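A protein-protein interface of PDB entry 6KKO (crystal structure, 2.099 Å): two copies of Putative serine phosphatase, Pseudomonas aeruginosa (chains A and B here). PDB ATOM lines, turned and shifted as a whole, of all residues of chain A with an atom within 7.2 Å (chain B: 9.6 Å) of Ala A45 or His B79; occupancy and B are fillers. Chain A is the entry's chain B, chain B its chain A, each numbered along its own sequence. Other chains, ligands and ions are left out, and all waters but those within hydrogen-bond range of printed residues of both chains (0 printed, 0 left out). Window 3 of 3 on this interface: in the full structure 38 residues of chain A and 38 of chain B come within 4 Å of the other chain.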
ATOM      1  N   LEU A  20     -19.074  26.260  18.908  1.00  0.00           N
ATOM      2  CA  LEU A  20     -17.780  25.653  19.177  1.00  0.00           C
ATOM      3  C   LEU A  20     -17.381  25.810  20.643  1.00  0.00           C
ATOM      4  O   LEU A  20     -16.882  24.865  21.263  1.00  0.00           O
ATOM      5  CB  LEU A  20     -16.717  26.298  18.282  1.00  0.00           C
ATOM      6  CG  LEU A  20     -17.169  26.653  16.869  1.00  0.00           C
ATOM      7  CD1 LEU A  20     -16.100  27.465  16.086  1.00  0.00           C
ATOM      8  CD2 LEU A  20     -17.712  25.401  16.105  1.00  0.00           C
ATOM      9  N   ALA A  38      -8.327  28.595  23.967  1.00  0.00           N
ATOM     10  CA  ALA A  38      -9.138  27.536  23.382  1.00  0.00           C
ATOM     11  C   ALA A  38      -9.635  27.947  22.002  1.00  0.00           C
ATOM     12  O   ALA A  38      -9.627  27.146  21.059  1.00  0.00           O
ATOM     13  CB  ALA A  38     -10.307  27.212  24.305  1.00  0.00           C
ATOM     14  N   LEU A  39     -10.053  29.204  21.864  1.00  0.00           N
ATOM     15  CA  LEU A  39     -10.477  29.714  20.567  1.00  0.00           C
ATOM     16  C   LEU A  39      -9.339  29.657  19.553  1.00  0.00           C
ATOM     17  O   LEU A  39      -9.527  29.203  18.417  1.00  0.00           O
ATOM     18  CB  LEU A  39     -10.995  31.140  20.735  1.00  0.00           C
ATOM     19  CG  LEU A  39     -11.380  31.904  19.474  1.00  0.00           C
ATOM     20  CD1 LEU A  39     -12.483  31.163  18.732  1.00  0.00           C
ATOM     21  CD2 LEU A  39     -11.822  33.300  19.881  1.00  0.00           C
ATOM     22  N   ARG A  40      -8.140  30.102  19.949  1.00  0.00           N
ATOM     23  CA  ARG A  40      -7.010  30.112  19.021  1.00  0.00           C
ATOM     24  C   ARG A  40      -6.613  28.701  18.605  1.00  0.00           C
ATOM     25  O   ARG A  40      -6.235  28.474  17.451  1.00  0.00           O
ATOM     26  CB  ARG A  40      -5.818  30.854  19.630  1.00  0.00           C
ATOM     27  CG  ARG A  40      -6.004  32.370  19.635  1.00  0.00           C
ATOM     28  CD  ARG A  40      -4.810  33.129  20.204  1.00  0.00           C
ATOM     29  NE  ARG A  40      -4.770  33.130  21.665  1.00  0.00           N
ATOM     30  CZ  ARG A  40      -3.917  32.416  22.394  1.00  0.00           C
ATOM     31  NH1 ARG A  40      -3.021  31.636  21.802  1.00  0.00           N
ATOM     32  NH2 ARG A  40      -3.956  32.488  23.714  1.00  0.00           N
ATOM     33  N   ASN A  41      -6.679  27.739  19.530  1.00  0.00           N
ATOM     34  CA  ASN A  41      -6.424  26.351  19.151  1.00  0.00           C
ATOM     35  C   ASN A  41      -7.494  25.837  18.200  1.00  0.00           C
ATOM     36  O   ASN A  41      -7.185  25.152  17.221  1.00  0.00           O
ATOM     37  CB  ASN A  41      -6.344  25.461  20.389  1.00  0.00           C
ATOM     38  CG  ASN A  41      -5.141  25.774  21.252  1.00  0.00           C
ATOM     39  OD1 ASN A  41      -4.173  26.373  20.788  1.00  0.00           O
ATOM     40  ND2 ASN A  41      -5.195  25.372  22.515  1.00  0.00           N
ATOM     41  N   TYR A  42      -8.761  26.162  18.467  1.00  0.00           N
ATOM     42  CA  TYR A  42      -9.828  25.688  17.592  1.00  0.00           C
ATOM     43  C   TYR A  42      -9.683  26.273  16.188  1.00  0.00           C
ATOM     44  O   TYR A  42      -9.901  25.575  15.189  1.00  0.00           O
ATOM     45  CB  TYR A  42     -11.192  26.057  18.173  1.00  0.00           C
ATOM     46  CG  TYR A  42     -12.336  25.260  17.583  1.00  0.00           C
ATOM     47  CD1 TYR A  42     -12.838  25.554  16.325  1.00  0.00           C
ATOM     48  CD2 TYR A  42     -12.955  24.254  18.315  1.00  0.00           C
ATOM     49  CE1 TYR A  42     -13.882  24.841  15.790  1.00  0.00           C
ATOM     50  CE2 TYR A  42     -14.009  23.536  17.786  1.00  0.00           C
ATOM     51  CZ  TYR A  42     -14.464  23.834  16.520  1.00  0.00           C
ATOM     52  OH  TYR A  42     -15.515  23.133  15.975  1.00  0.00           O
ATOM     53  N   LEU A  43      -9.327  27.560  16.091  1.00  0.00           N
ATOM     54  CA  LEU A  43      -9.149  28.178  14.778  1.00  0.00           C
ATOM     55  C   LEU A  43      -8.007  27.523  14.008  1.00  0.00           C
ATOM     56  O   LEU A  43      -8.107  27.319  12.793  1.00  0.00           O
ATOM     57  CB  LEU A  43      -8.915  29.680  14.942  1.00  0.00           C
ATOM     58  CG  LEU A  43     -10.138  30.427  15.480  1.00  0.00           C
ATOM     59  CD1 LEU A  43      -9.742  31.796  16.020  1.00  0.00           C
ATOM     60  CD2 LEU A  43     -11.220  30.550  14.405  1.00  0.00           C
ATOM     61  N   HIS A  44      -6.920  27.166  14.699  1.00  0.00           N
ATOM     62  CA  HIS A  44      -5.828  26.464  14.033  1.00  0.00           C
ATOM     63  C   HIS A  44      -6.244  25.062  13.605  1.00  0.00           C
ATOM     64  O   HIS A  44      -5.923  24.626  12.493  1.00  0.00           O
ATOM     65  CB  HIS A  44      -4.607  26.395  14.946  1.00  0.00           C
ATOM     66  CG  HIS A  44      -3.484  25.584  14.380  1.00  0.00           C
ATOM     67  ND1 HIS A  44      -2.993  25.778  13.107  1.00  0.00           N
ATOM     68  CD2 HIS A  44      -2.767  24.561  14.907  1.00  0.00           C
ATOM     69  CE1 HIS A  44      -2.016  24.919  12.877  1.00  0.00           C
ATOM     70  NE2 HIS A  44      -1.861  24.169  13.953  1.00  0.00           N
ATOM     71  N   ALA A  45      -6.974  24.351  14.465  1.00  0.00           N
ATOM     72  CA  ALA A  45      -7.385  22.990  14.142  1.00  0.00           C
ATOM     73  C   ALA A  45      -8.348  22.966  12.965  1.00  0.00           C
ATOM     74  O   ALA A  45      -8.397  21.972  12.224  1.00  0.00           O
ATOM     75  CB  ALA A  45      -8.018  22.334  15.369  1.00  0.00           C
ATOM     76  N   GLU A  46      -9.101  24.053  12.752  1.00  0.00           N
ATOM     77  CA  GLU A  46      -9.973  24.176  11.589  1.00  0.00           C
ATOM     78  C   GLU A  46      -9.270  24.877  10.430  1.00  0.00           C
ATOM     79  O   GLU A  46      -9.926  25.240   9.449  1.00  0.00           O
ATOM     80  CB  GLU A  46     -11.271  24.918  11.941  1.00  0.00           C
ATOM     81  CG  GLU A  46     -12.103  24.246  13.024  1.00  0.00           C
ATOM     82  CD  GLU A  46     -12.771  22.973  12.536  1.00  0.00           C
ATOM     83  OE1 GLU A  46     -13.203  22.159  13.356  1.00  0.00           O
ATOM     84  OE2 GLU A  46     -12.882  22.783  11.321  1.00  0.00           O
ATOM     85  N   GLN A  47      -7.943  25.040  10.512  1.00  0.00           N
ATOM     86  CA  GLN A  47      -7.137  25.625   9.441  1.00  0.00           C
ATOM     87  C   GLN A  47      -7.717  26.962   9.001  1.00  0.00           C
ATOM     88  O   GLN A  47      -7.815  27.263   7.810  1.00  0.00           O
ATOM     89  CB  GLN A  47      -6.990  24.657   8.265  1.00  0.00           C
ATOM     90  CG  GLN A  47      -5.586  24.063   8.170  1.00  0.00           C
ATOM     91  CD  GLN A  47      -5.509  22.844   7.277  1.00  0.00           C
ATOM     92  OE1 GLN A  47      -6.517  22.390   6.731  1.00  0.00           O
ATOM     93  NE2 GLN A  47      -4.306  22.302   7.126  1.00  0.00           N
ATOM     94  N   ALA A  48      -8.102  27.778   9.976  1.00  0.00           N
ATOM     95  CA  ALA A  48      -8.553  29.120   9.657  1.00  0.00           C
ATOM     96  C   ALA A  48      -7.409  29.884   9.014  1.00  0.00           C
ATOM     97  O   ALA A  48      -6.261  29.806   9.462  1.00  0.00           O
ATOM     98  CB  ALA A  48      -9.040  29.844  10.914  1.00  0.00           C
ATOM     99  N   TYR A  95     -17.531  32.456  10.923  1.00  0.00           N
ATOM    100  CA  TYR A  95     -17.641  32.384  12.369  1.00  0.00           C
ATOM    101  C   TYR A  95     -18.602  33.450  12.885  1.00  0.00           C
ATOM    102  O   TYR A  95     -18.770  34.519  12.286  1.00  0.00           O
ATOM    103  CB  TYR A  95     -16.266  32.540  13.012  1.00  0.00           C
ATOM    104  CG  TYR A  95     -15.380  31.340  12.779  1.00  0.00           C
ATOM    105  CD1 TYR A  95     -14.612  31.228  11.627  1.00  0.00           C
ATOM    106  CD2 TYR A  95     -15.321  30.310  13.706  1.00  0.00           C
ATOM    107  CE1 TYR A  95     -13.806  30.121  11.409  1.00  0.00           C
ATOM    108  CE2 TYR A  95     -14.521  29.207  13.499  1.00  0.00           C
ATOM    109  CZ  TYR A  95     -13.766  29.113  12.354  1.00  0.00           C
ATOM    110  OH  TYR A  95     -12.972  28.000  12.164  1.00  0.00           O
ATOM    111  N   GLY B  25     -17.078  23.097  25.359  1.00  0.00           N
ATOM    112  CA  GLY B  25     -16.026  23.176  24.374  1.00  0.00           C
ATOM    113  C   GLY B  25     -14.786  22.420  24.801  1.00  0.00           C
ATOM    114  O   GLY B  25     -14.783  21.708  25.812  1.00  0.00           O
ATOM    115  N   PRO B  26     -13.704  22.563  24.033  1.00  0.00           N
ATOM    116  CA  PRO B  26     -12.435  21.939  24.425  1.00  0.00           C
ATOM    117  C   PRO B  26     -12.002  22.414  25.803  1.00  0.00           C
ATOM    118  O   PRO B  26     -12.086  23.600  26.133  1.00  0.00           O
ATOM    119  CB  PRO B  26     -11.459  22.401  23.338  1.00  0.00           C
ATOM    120  CG  PRO B  26     -12.329  22.691  22.163  1.00  0.00           C
ATOM    121  CD  PRO B  26     -13.603  23.249  22.735  1.00  0.00           C
ATOM    122  N   ILE B  27     -11.557  21.469  26.623  1.00  0.00           N
ATOM    123  CA  ILE B  27     -11.280  21.751  28.022  1.00  0.00           C
ATOM    124  C   ILE B  27      -9.843  21.341  28.322  1.00  0.00           C
ATOM    125  O   ILE B  27      -9.481  20.162  28.213  1.00  0.00           O
ATOM    126  CB  ILE B  27     -12.292  21.050  28.942  1.00  0.00           C
ATOM    127  CG1 ILE B  27     -11.927  21.282  30.395  1.00  0.00           C
ATOM    128  CG2 ILE B  27     -12.404  19.560  28.619  1.00  0.00           C
ATOM    129  CD1 ILE B  27     -11.952  22.734  30.795  1.00  0.00           C
ATOM    130  N   SER B  28      -9.022  22.323  28.671  1.00  0.00           N
ATOM    131  CA  SER B  28      -7.611  22.112  28.927  1.00  0.00           C
ATOM    132  C   SER B  28      -7.339  22.146  30.424  1.00  0.00           C
ATOM    133  O   SER B  28      -8.159  22.603  31.225  1.00  0.00           O
ATOM    134  CB  SER B  28      -6.769  23.179  28.233  1.00  0.00           C
ATOM    135  OG  SER B  28      -6.937  24.433  28.871  1.00  0.00           O
ATOM    136  N   ARG B  68     -10.544  14.549  31.304  1.00  0.00           N
ATOM    137  CA  ARG B  68      -9.184  14.662  30.790  1.00  0.00           C
ATOM    138  C   ARG B  68      -8.506  13.303  30.714  1.00  0.00           C
ATOM    139  O   ARG B  68      -7.866  12.981  29.707  1.00  0.00           O
ATOM    140  CB  ARG B  68      -8.372  15.609  31.664  1.00  0.00           C
ATOM    141  CG  ARG B  68      -8.892  17.026  31.661  1.00  0.00           C
ATOM    142  CD  ARG B  68      -8.373  17.743  30.448  1.00  0.00           C
ATOM    143  NE  ARG B  68      -6.915  17.744  30.457  1.00  0.00           N
ATOM    144  CZ  ARG B  68      -6.168  18.038  29.401  1.00  0.00           C
ATOM    145  NH1 ARG B  68      -6.745  18.356  28.250  1.00  0.00           N
ATOM    146  NH2 ARG B  68      -4.847  18.016  29.500  1.00  0.00           N
ATOM    147  N   ALA B  71      -9.948  11.238  27.811  1.00  0.00           N
ATOM    148  CA  ALA B  71      -9.512  11.752  26.516  1.00  0.00           C
ATOM    149  C   ALA B  71      -8.058  11.389  26.239  1.00  0.00           C
ATOM    150  O   ALA B  71      -7.693  11.094  25.097  1.00  0.00           O
ATOM    151  CB  ALA B  71      -9.704  13.268  26.460  1.00  0.00           C
ATOM    152  N   GLY B  75      -6.498   8.612  23.390  1.00  0.00           N
ATOM    153  CA  GLY B  75      -5.648   9.292  22.441  1.00  0.00           C
ATOM    154  C   GLY B  75      -6.119  10.653  21.982  1.00  0.00           C
ATOM    155  O   GLY B  75      -5.361  11.335  21.281  1.00  0.00           O
ATOM    156  N   TYR B  76      -7.335  11.077  22.345  1.00  0.00           N
ATOM    157  CA  TYR B  76      -7.870  12.353  21.878  1.00  0.00           C
ATOM    158  C   TYR B  76      -6.863  13.475  22.110  1.00  0.00           C
ATOM    159  O   TYR B  76      -6.077  13.447  23.062  1.00  0.00           O
ATOM    160  CB  TYR B  76      -9.176  12.710  22.598  1.00  0.00           C
ATOM    161  CG  TYR B  76     -10.304  11.699  22.517  1.00  0.00           C
ATOM    162  CD1 TYR B  76     -10.350  10.731  21.521  1.00  0.00           C
ATOM    163  CD2 TYR B  76     -11.342  11.733  23.442  1.00  0.00           C
ATOM    164  CE1 TYR B  76     -11.397   9.816  21.461  1.00  0.00           C
ATOM    165  CE2 TYR B  76     -12.386  10.830  23.390  1.00  0.00           C
ATOM    166  CZ  TYR B  76     -12.412   9.874  22.401  1.00  0.00           C
ATOM    167  OH  TYR B  76     -13.461   8.978  22.364  1.00  0.00           O
ATOM    168  N   GLY B  77      -6.924  14.432  21.200  1.00  0.00           N
ATOM    169  CA  GLY B  77      -6.115  15.632  21.163  1.00  0.00           C
ATOM    170  C   GLY B  77      -6.765  16.793  21.867  1.00  0.00           C
ATOM    171  O   GLY B  77      -7.868  16.718  22.341  1.00  0.00           O
ATOM    172  N   GLU B  78      -6.060  17.897  21.912  1.00  0.00           N
ATOM    173  CA  GLU B  78      -6.561  19.067  22.594  1.00  0.00           C
ATOM    174  C   GLU B  78      -7.862  19.448  21.983  1.00  0.00           C
ATOM    175  O   GLU B  78      -8.786  19.772  22.671  1.00  0.00           O
ATOM    176  CB  GLU B  78      -5.574  20.216  22.416  1.00  0.00           C
ATOM    177  N   HIS B  79      -7.931  19.390  20.669  1.00  0.00           N
ATOM    178  CA  HIS B  79      -9.162  19.716  19.959  1.00  0.00           C
ATOM    179  C   HIS B  79     -10.306  18.771  20.259  1.00  0.00           C
ATOM    180  O   HIS B  79     -11.424  19.186  20.351  1.00  0.00           O
ATOM    181  CB  HIS B  79      -8.901  19.737  18.468  1.00  0.00           C
ATOM    182  CG  HIS B  79      -9.971  20.404  17.682  1.00  0.00           C
ATOM    183  ND1 HIS B  79     -10.682  19.755  16.704  1.00  0.00           N
ATOM    184  CD2 HIS B  79     -10.448  21.663  17.717  1.00  0.00           C
ATOM    185  CE1 HIS B  79     -11.552  20.587  16.168  1.00  0.00           C
ATOM    186  NE2 HIS B  79     -11.430  21.751  16.769  1.00  0.00           N
ATOM    187  N   GLU B  80      -9.995  17.485  20.345  1.00  0.00           N
ATOM    188  CA  GLU B  80     -10.966  16.449  20.640  1.00  0.00           C
ATOM    189  C   GLU B  80     -11.447  16.350  22.109  1.00  0.00           C
ATOM    190  O   GLU B  80     -12.556  15.885  22.380  1.00  0.00           O
ATOM    191  CB  GLU B  80     -10.515  15.105  20.087  1.00  0.00           C
ATOM    192  CG  GLU B  80     -11.645  14.211  19.595  1.00  0.00           C
ATOM    193  CD  GLU B  80     -12.333  14.708  18.345  1.00  0.00           C
ATOM    194  OE1 GLU B  80     -12.008  15.801  17.861  1.00  0.00           O
ATOM    195  OE2 GLU B  80     -13.197  13.991  17.818  1.00  0.00           O
ATOM    196  N   ALA B  81     -10.604  16.776  23.043  1.00  0.00           N
ATOM    197  CA  ALA B  81     -10.912  16.697  24.472  1.00  0.00           C
ATOM    198  C   ALA B  81     -11.933  17.783  24.811  1.00  0.00           C
ATOM    199  O   ALA B  81     -11.613  18.848  25.346  1.00  0.00           O
ATOM    200  CB  ALA B  81      -9.645  16.829  25.308  1.00  0.00           C
ATOM    201  N   ALA B  82     -13.195  17.486  24.500  1.00  0.00           N
ATOM    202  CA  ALA B  82     -14.307  18.413  24.636  1.00  0.00           C
ATOM    203  C   ALA B  82     -15.218  17.975  25.776  1.00  0.00           C
ATOM    204  O   ALA B  82     -15.258  16.797  26.149  1.00  0.00           O
ATOM    205  CB  ALA B  82     -15.111  18.501  23.334  1.00  0.00           C
ATOM    206  N   ALA B  83     -15.963  18.934  26.324  1.00  0.00           N
ATOM    207  CA  ALA B  83     -16.801  18.639  27.479  1.00  0.00           C
ATOM    208  C   ALA B  83     -17.845  19.729  27.674  1.00  0.00           C
ATOM    209  O   ALA B  83     -17.728  20.841  27.149  1.00  0.00           O
ATOM    210  CB  ALA B  83     -15.960  18.481  28.748  1.00  0.00           C
ATOM    211  N   LEU B 102     -18.293  13.003  25.391  1.00  0.00           N
ATOM    212  CA  LEU B 102     -18.512  11.927  24.433  1.00  0.00           C
ATOM    213  C   LEU B 102     -17.578  10.769  24.745  1.00  0.00           C
ATOM    214  O   LEU B 102     -16.394  10.969  25.030  1.00  0.00           O
ATOM    215  CB  LEU B 102     -18.303  12.404  22.994  1.00  0.00           C
ATOM    216  CG  LEU B 102     -19.372  13.378  22.492  1.00  0.00           C
ATOM    217  CD1 LEU B 102     -18.904  14.127  21.260  1.00  0.00           C
ATOM    218  CD2 LEU B 102     -20.679  12.657  22.215  1.00  0.00           C
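No position is printed for both chains.
CA of Gly B25 touches O of Leu A20 (3.6 Å).
Pro B26 touches Leu A20 (CD to O, 3.9 Å).
CE2 of Tyr A42 touches NE2 of His B79, at 3.3 Å.
Ala A45 touches His B79.
Glu A46 touches His B79.
The backbone carbonyl oxygen (O) of Ala B83 lies within hydrogen-bond range of the backbone NH (N) of Gly B25, 3.0 Å away.
Ala A45 touches just one residue of chain B: His B79.
Printed residues of chain A within 4 Å of His B79: Tyr A42, Ala A45 and Glu A46.
Of chain B, only His B79 (3.3 Å) comes within 4 Å of Tyr A42.
No residue of chain B comes within 4 Å of His A44.
No residue of chain A comes within 4 Å of Glu B78.
Of the printed residues of chain A, Pro B26 touches Leu A20 (3.9 Å).
Printed residues of chain A within 4 Å of Gly B25: Leu A20.
Of the printed residues of chain B, Leu A20 touches Gly B25 and Pro B26.
Gly B77 touches none of the printed residues of chain A.
The nearest printed residue of chain B that does not touch Ala A45 is Glu B78 (7.2 Å).
The nearest printed residue of chain A that does not touch Gly B25 is Ala A38 (6.6 Å).
Printed residues of chain A that touch a printed residue of chain B: Leu A20, Tyr A42, Ala A45 and Glu A46.
Hydrophobic or aromatic side chains of chain A within 4 Å of the printed part of chain B: Tyr A42 and Ala A45.
Hydrophobic or aromatic side chains of chain B that line the printed part of chain A: Pro B26 and His B79.
Among the printed residues, 5 pairs touch across the chains.
Among the printed residues, no Asp or Glu carboxylate lies within 4 Å of a Lys or Arg side-chain nitrogen of the other chain.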
